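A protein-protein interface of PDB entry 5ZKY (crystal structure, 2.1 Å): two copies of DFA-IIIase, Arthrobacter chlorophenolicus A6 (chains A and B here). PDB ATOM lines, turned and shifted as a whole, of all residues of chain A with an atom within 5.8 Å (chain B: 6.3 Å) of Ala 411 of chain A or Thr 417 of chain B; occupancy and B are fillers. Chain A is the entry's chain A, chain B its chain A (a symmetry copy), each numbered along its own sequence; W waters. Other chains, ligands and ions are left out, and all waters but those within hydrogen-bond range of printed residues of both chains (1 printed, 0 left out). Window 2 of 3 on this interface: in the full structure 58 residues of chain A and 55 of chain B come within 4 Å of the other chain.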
ATOM      1  N   ARG A 391      17.940  11.394  -6.278  1.00  0.00           N
ATOM      2  CA  ARG A 391      18.561  10.133  -5.909  1.00  0.00           C
ATOM      3  C   ARG A 391      19.507  10.315  -4.719  1.00  0.00           C
ATOM      4  O   ARG A 391      20.553   9.704  -4.647  1.00  0.00           O
ATOM      5  CB  ARG A 391      19.228   9.485  -7.134  1.00  0.00           C
ATOM      6  CG  ARG A 391      18.250   9.345  -8.313  1.00  0.00           C
ATOM      7  CD  ARG A 391      18.851   8.582  -9.474  1.00  0.00           C
ATOM      8  NE  ARG A 391      19.056   7.169  -9.138  1.00  0.00           N
ATOM      9  CZ  ARG A 391      19.327   6.193 -10.013  1.00  0.00           C
ATOM     10  NH1 ARG A 391      19.427   6.438 -11.322  1.00  0.00           N
ATOM     11  NH2 ARG A 391      19.493   4.945  -9.574  1.00  0.00           N
ATOM     12  N   ASN A 392      19.094  11.167  -3.789  1.00  0.00           N
ATOM     13  CA  ASN A 392      19.806  11.408  -2.535  1.00  0.00           C
ATOM     14  C   ASN A 392      19.203  10.522  -1.463  1.00  0.00           C
ATOM     15  O   ASN A 392      18.075  10.039  -1.610  1.00  0.00           O
ATOM     16  CB  ASN A 392      19.686  12.893  -2.141  1.00  0.00           C
ATOM     17  CG  ASN A 392      20.208  13.815  -3.222  1.00  0.00           C
ATOM     18  OD1 ASN A 392      21.404  13.790  -3.530  1.00  0.00           O
ATOM     19  ND2 ASN A 392      19.318  14.605  -3.831  1.00  0.00           N
ATOM     20  N   THR A 393      19.959  10.310  -0.395  1.00  0.00           N
ATOM     21  CA  THR A 393      19.491   9.554   0.756  1.00  0.00           C
ATOM     22  C   THR A 393      19.562  10.455   1.982  1.00  0.00           C
ATOM     23  O   THR A 393      20.629  10.991   2.305  1.00  0.00           O
ATOM     24  CB  THR A 393      20.324   8.293   0.950  1.00  0.00           C
ATOM     25  OG1 THR A 393      20.163   7.471  -0.203  1.00  0.00           O
ATOM     26  CG2 THR A 393      19.867   7.513   2.175  1.00  0.00           C
ATOM     27  N   ILE A 394      18.416  10.639   2.640  1.00  0.00           N
ATOM     28  CA  ILE A 394      18.288  11.558   3.766  1.00  0.00           C
ATOM     29  C   ILE A 394      17.710  10.829   4.974  1.00  0.00           C
ATOM     30  O   ILE A 394      16.537  10.449   4.986  1.00  0.00           O
ATOM     31  CB  ILE A 394      17.494  12.819   3.378  1.00  0.00           C
ATOM     32  CG1 ILE A 394      18.272  13.574   2.283  1.00  0.00           C
ATOM     33  CG2 ILE A 394      17.317  13.734   4.594  1.00  0.00           C
ATOM     34  CD1 ILE A 394      17.429  14.501   1.493  1.00  0.00           C
ATOM     35  N   LEU A 395      18.556  10.632   5.982  1.00  0.00           N
ATOM     36  CA  LEU A 395      18.211   9.829   7.144  1.00  0.00           C
ATOM     37  C   LEU A 395      18.366  10.630   8.431  1.00  0.00           C
ATOM     38  O   LEU A 395      19.363  11.322   8.604  1.00  0.00           O
ATOM     39  CB  LEU A 395      19.123   8.621   7.214  1.00  0.00           C
ATOM     40  CG  LEU A 395      19.330   7.787   5.954  1.00  0.00           C
ATOM     41  CD1 LEU A 395      20.318   6.681   6.272  1.00  0.00           C
ATOM     42  CD2 LEU A 395      18.019   7.194   5.440  1.00  0.00           C
ATOM     43  N   ARG A 407       9.805  12.503  -2.457  1.00  0.00           N
ATOM     44  CA  ARG A 407       9.933  11.113  -1.991  1.00  0.00           C
ATOM     45  C   ARG A 407       9.979  10.057  -3.100  1.00  0.00           C
ATOM     46  O   ARG A 407      10.434   8.936  -2.852  1.00  0.00           O
ATOM     47  CB  ARG A 407       8.801  10.747  -0.999  1.00  0.00           C
ATOM     48  CG  ARG A 407       9.119  11.020   0.471  1.00  0.00           C
ATOM     49  CD  ARG A 407       9.382  12.486   0.732  1.00  0.00           C
ATOM     50  NE  ARG A 407       9.401  12.777   2.159  1.00  0.00           N
ATOM     51  CZ  ARG A 407       9.640  13.976   2.682  1.00  0.00           C
ATOM     52  NH1 ARG A 407       9.903  15.020   1.895  1.00  0.00           N
ATOM     53  NH2 ARG A 407       9.617  14.135   4.005  1.00  0.00           N
ATOM     54  N   VAL A 409      11.841  10.141  -5.795  1.00  0.00           N
ATOM     55  CA  VAL A 409      13.203  10.030  -6.346  1.00  0.00           C
ATOM     56  C   VAL A 409      14.307  10.263  -5.307  1.00  0.00           C
ATOM     57  O   VAL A 409      15.451  10.430  -5.677  1.00  0.00           O
ATOM     58  CB  VAL A 409      13.399  10.984  -7.559  1.00  0.00           C
ATOM     59  CG1 VAL A 409      12.516  10.544  -8.738  1.00  0.00           C
ATOM     60  CG2 VAL A 409      13.107  12.434  -7.190  1.00  0.00           C
ATOM     61  N   ASN A 410      13.961  10.273  -4.021  1.00  0.00           N
ATOM     62  CA  ASN A 410      14.945  10.322  -2.937  1.00  0.00           C
ATOM     63  C   ASN A 410      14.521   9.351  -1.852  1.00  0.00           C
ATOM     64  O   ASN A 410      13.321   9.177  -1.604  1.00  0.00           O
ATOM     65  CB  ASN A 410      15.025  11.729  -2.335  1.00  0.00           C
ATOM     66  CG  ASN A 410      15.475  12.765  -3.336  1.00  0.00           C
ATOM     67  OD1 ASN A 410      16.670  12.913  -3.599  1.00  0.00           O
ATOM     68  ND2 ASN A 410      14.516  13.491  -3.906  1.00  0.00           N
ATOM     69  N   ALA A 411      15.501   8.729  -1.203  1.00  0.00           N
ATOM     70  CA  ALA A 411      15.248   7.841  -0.070  1.00  0.00           C
ATOM     71  C   ALA A 411      15.270   8.662   1.221  1.00  0.00           C
ATOM     72  O   ALA A 411      16.318   9.166   1.611  1.00  0.00           O
ATOM     73  CB  ALA A 411      16.294   6.733  -0.030  1.00  0.00           C
ATOM     74  N   ILE A 412      14.113   8.812   1.862  1.00  0.00           N
ATOM     75  CA  ILE A 412      13.984   9.628   3.071  1.00  0.00           C
ATOM     76  C   ILE A 412      13.563   8.746   4.248  1.00  0.00           C
ATOM     77  O   ILE A 412      12.587   8.017   4.152  1.00  0.00           O
ATOM     78  CB  ILE A 412      12.965  10.794   2.882  1.00  0.00           C
ATOM     79  CG1 ILE A 412      13.605  12.010   2.220  1.00  0.00           C
ATOM     80  CG2 ILE A 412      12.490  11.342   4.227  1.00  0.00           C
ATOM     81  CD1 ILE A 412      13.899  11.869   0.780  1.00  0.00           C
ATOM     82  N   ARG A 413      14.294   8.816   5.357  1.00  0.00           N
ATOM     83  CA  ARG A 413      13.774   8.337   6.643  1.00  0.00           C
ATOM     84  C   ARG A 413      13.707   9.509   7.597  1.00  0.00           C
ATOM     85  O   ARG A 413      14.728  10.140   7.919  1.00  0.00           O
ATOM     86  CB  ARG A 413      14.626   7.232   7.249  1.00  0.00           C
ATOM     87  CG  ARG A 413      14.034   6.652   8.538  1.00  0.00           C
ATOM     88  CD  ARG A 413      14.847   5.461   9.009  1.00  0.00           C
ATOM     89  NE  ARG A 413      16.179   5.881   9.461  1.00  0.00           N
ATOM     90  CZ  ARG A 413      17.333   5.241   9.219  1.00  0.00           C
ATOM     91  NH1 ARG A 413      17.379   4.124   8.503  1.00  0.00           N
ATOM     92  NH2 ARG A 413      18.469   5.733   9.709  1.00  0.00           N
ATOM     93  N   SER B 399      22.285  -1.185   0.930  1.00  0.00           N
ATOM     94  CA  SER B 399      21.040  -1.945   0.711  1.00  0.00           C
ATOM     95  C   SER B 399      21.263  -3.403   1.085  1.00  0.00           C
ATOM     96  O   SER B 399      22.401  -3.821   1.361  1.00  0.00           O
ATOM     97  CB  SER B 399      20.606  -1.863  -0.757  1.00  0.00           C
ATOM     98  OG  SER B 399      21.514  -2.579  -1.569  1.00  0.00           O
ATOM     99  N   GLN B 402      23.819  -5.105  -1.000  1.00  0.00           N
ATOM    100  CA  GLN B 402      25.164  -4.586  -0.720  1.00  0.00           C
ATOM    101  C   GLN B 402      25.780  -5.037   0.611  1.00  0.00           C
ATOM    102  O   GLN B 402      26.971  -4.810   0.847  1.00  0.00           O
ATOM    103  CB  GLN B 402      25.112  -3.061  -0.776  1.00  0.00           C
ATOM    104  CG  GLN B 402      24.733  -2.544  -2.158  1.00  0.00           C
ATOM    105  CD  GLN B 402      24.425  -1.068  -2.169  1.00  0.00           C
ATOM    106  OE1 GLN B 402      24.080  -0.483  -1.145  1.00  0.00           O
ATOM    107  NE2 GLN B 402      24.536  -0.456  -3.343  1.00  0.00           N
ATOM    108  N   ALA B 414      19.103  -2.360   6.392  1.00  0.00           N
ATOM    109  CA  ALA B 414      19.424  -1.875   5.066  1.00  0.00           C
ATOM    110  C   ALA B 414      19.180  -0.372   5.008  1.00  0.00           C
ATOM    111  O   ALA B 414      18.207   0.146   5.579  1.00  0.00           O
ATOM    112  CB  ALA B 414      18.570  -2.590   4.010  1.00  0.00           C
ATOM    113  N   THR B 415      20.094   0.330   4.353  1.00  0.00           N
ATOM    114  CA  THR B 415      19.872   1.719   4.004  1.00  0.00           C
ATOM    115  C   THR B 415      18.572   1.789   3.190  1.00  0.00           C
ATOM    116  O   THR B 415      18.436   1.044   2.236  1.00  0.00           O
ATOM    117  CB  THR B 415      21.025   2.238   3.130  1.00  0.00           C
ATOM    118  OG1 THR B 415      22.262   2.128   3.854  1.00  0.00           O
ATOM    119  CG2 THR B 415      20.788   3.685   2.719  1.00  0.00           C
ATOM    120  N   PRO B 416      17.618   2.663   3.569  1.00  0.00           N
ATOM    121  CA  PRO B 416      16.415   2.822   2.730  1.00  0.00           C
ATOM    122  C   PRO B 416      16.776   3.210   1.287  1.00  0.00           C
ATOM    123  O   PRO B 416      17.769   3.906   1.077  1.00  0.00           O
ATOM    124  CB  PRO B 416      15.640   3.951   3.431  1.00  0.00           C
ATOM    125  CG  PRO B 416      16.106   3.909   4.851  1.00  0.00           C
ATOM    126  CD  PRO B 416      17.532   3.443   4.817  1.00  0.00           C
ATOM    127  N   THR B 417      15.999   2.746   0.310  1.00  0.00           N
ATOM    128  CA  THR B 417      16.317   2.994  -1.112  1.00  0.00           C
ATOM    129  C   THR B 417      15.203   3.707  -1.871  1.00  0.00           C
ATOM    130  O   THR B 417      14.073   3.728  -1.408  1.00  0.00           O
ATOM    131  CB  THR B 417      16.674   1.685  -1.832  1.00  0.00           C
ATOM    132  OG1 THR B 417      15.829   0.629  -1.353  1.00  0.00           O
ATOM    133  CG2 THR B 417      18.153   1.329  -1.582  1.00  0.00           C
ATOM    134  N   VAL B 418      15.568   4.310  -3.012  1.00  0.00           N
ATOM    135  CA  VAL B 418      14.647   4.890  -4.029  1.00  0.00           C
ATOM    136  C   VAL B 418      13.757   6.022  -3.485  1.00  0.00           C
ATOM    137  O   VAL B 418      12.635   5.802  -3.033  1.00  0.00           O
ATOM    138  CB  VAL B 418      13.857   3.768  -4.780  1.00  0.00           C
ATOM    139  CG1 VAL B 418      12.713   4.304  -5.637  1.00  0.00           C
ATOM    140  CG2 VAL B 418      14.813   2.967  -5.665  1.00  0.00           C
HETATM  141  O   HOH W   1      19.315   4.946  -0.680  1.00  0.00           O
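N of Arg 413 of chain A is in hydrogen-bond range of O of Ile 394 of chain A, 2.8 Å away.
N of Arg 391 of chain A lies within hydrogen-bond range of OD1 of Asn 410 of chain A (3.3 Å).
OD1 of Asn 410 of chain A sits at hydrogen-bond distance from N of Asn 392 of chain A (3.0 Å).
O of Asn 392 of chain A is in hydrogen-bond range of N of Ala 411 of chain A, at 2.9 Å.
N of Ile 394 of chain A sits at hydrogen-bond distance from O of Ala 411 of chain A, at 2.8 Å.
Among the printed residues, merely in contact across the chains: Thr 393 of chain A with Thr 415 of chain B (3.97 Å), Leu 395 of chain A with Pro 416 of chain B (3.8 Å), Arg 407 of chain A with Val 418 of chain B (3.8 Å), Asn 410 of chain A with Val 418 of chain B (3.7 Å), Ala 411 of chain A with Pro 416 of chain B (3.4 Å), Ala 411 of chain A with Thr 417 of chain B (3.7 Å), Ala 411 of chain A with Val 418 of chain B (3.9 Å) and Arg 413 of chain A with Pro 416 of chain B (3.8 Å).
Asn 392 of chain A touches none of the printed residues of chain B.
Printed residues of chain B within 4 Å of Leu 395 of chain A: Pro 416.
Printed residues of chain B within 4 Å of Arg 407 of chain A: Val 418 (3.8 Å).
Ala 411 of chain A touches just these residues of chain B: Pro 416, Thr 417 and Val 418.
Of the printed residues of chain B, Arg 413 of chain A touches Pro 416 (3.8 Å).
Printed residues of chain A within 4 Å of Thr 415 of chain B: Thr 393.
Of the printed residues of chain A, Pro 416 of chain B touches Leu 395 (3.8 Å), Ala 411 (3.4 Å) and Arg 413 (3.8 Å).
Printed residues of chain A within 4 Å of Thr 417 of chain B: Ala 411.
The nearest residue of chain B that does not touch Ala 411 of chain A is Thr 415 of chain B (6.1 Å).
Hydrophobic or aromatic side chains of chain B that line the printed part of chain A: Pro 416.
Of the 11 printed residues of chain A, 6 touch a printed residue of chain B.
Printed residues of chain A that touch a printed residue of chain B: Thr 393, Leu 395, Arg 407, Asn 410, Ala 411 and Arg 413.
Hydrophobic or aromatic side chains of chain A that line the printed part of chain B: Leu 395 and Ala 411.
Along chain A the printed residues that touch a printed residue of chain B span positions 393 to 413.
Among the printed residues, 8 pairs touch across the chains.
Among the printed residues, no Asp or Glu carboxylate lies within 4 Å of a Lys or Arg side-chain nitrogen of the other chain.
No position is printed for both chains.
Water W1 bridges the backbone carbonyl oxygen (O) of Pro 416 of chain B (2.6 Å) and the side-chain hydroxyl (OG1) of Thr 393 of chain A (2.7 Å).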
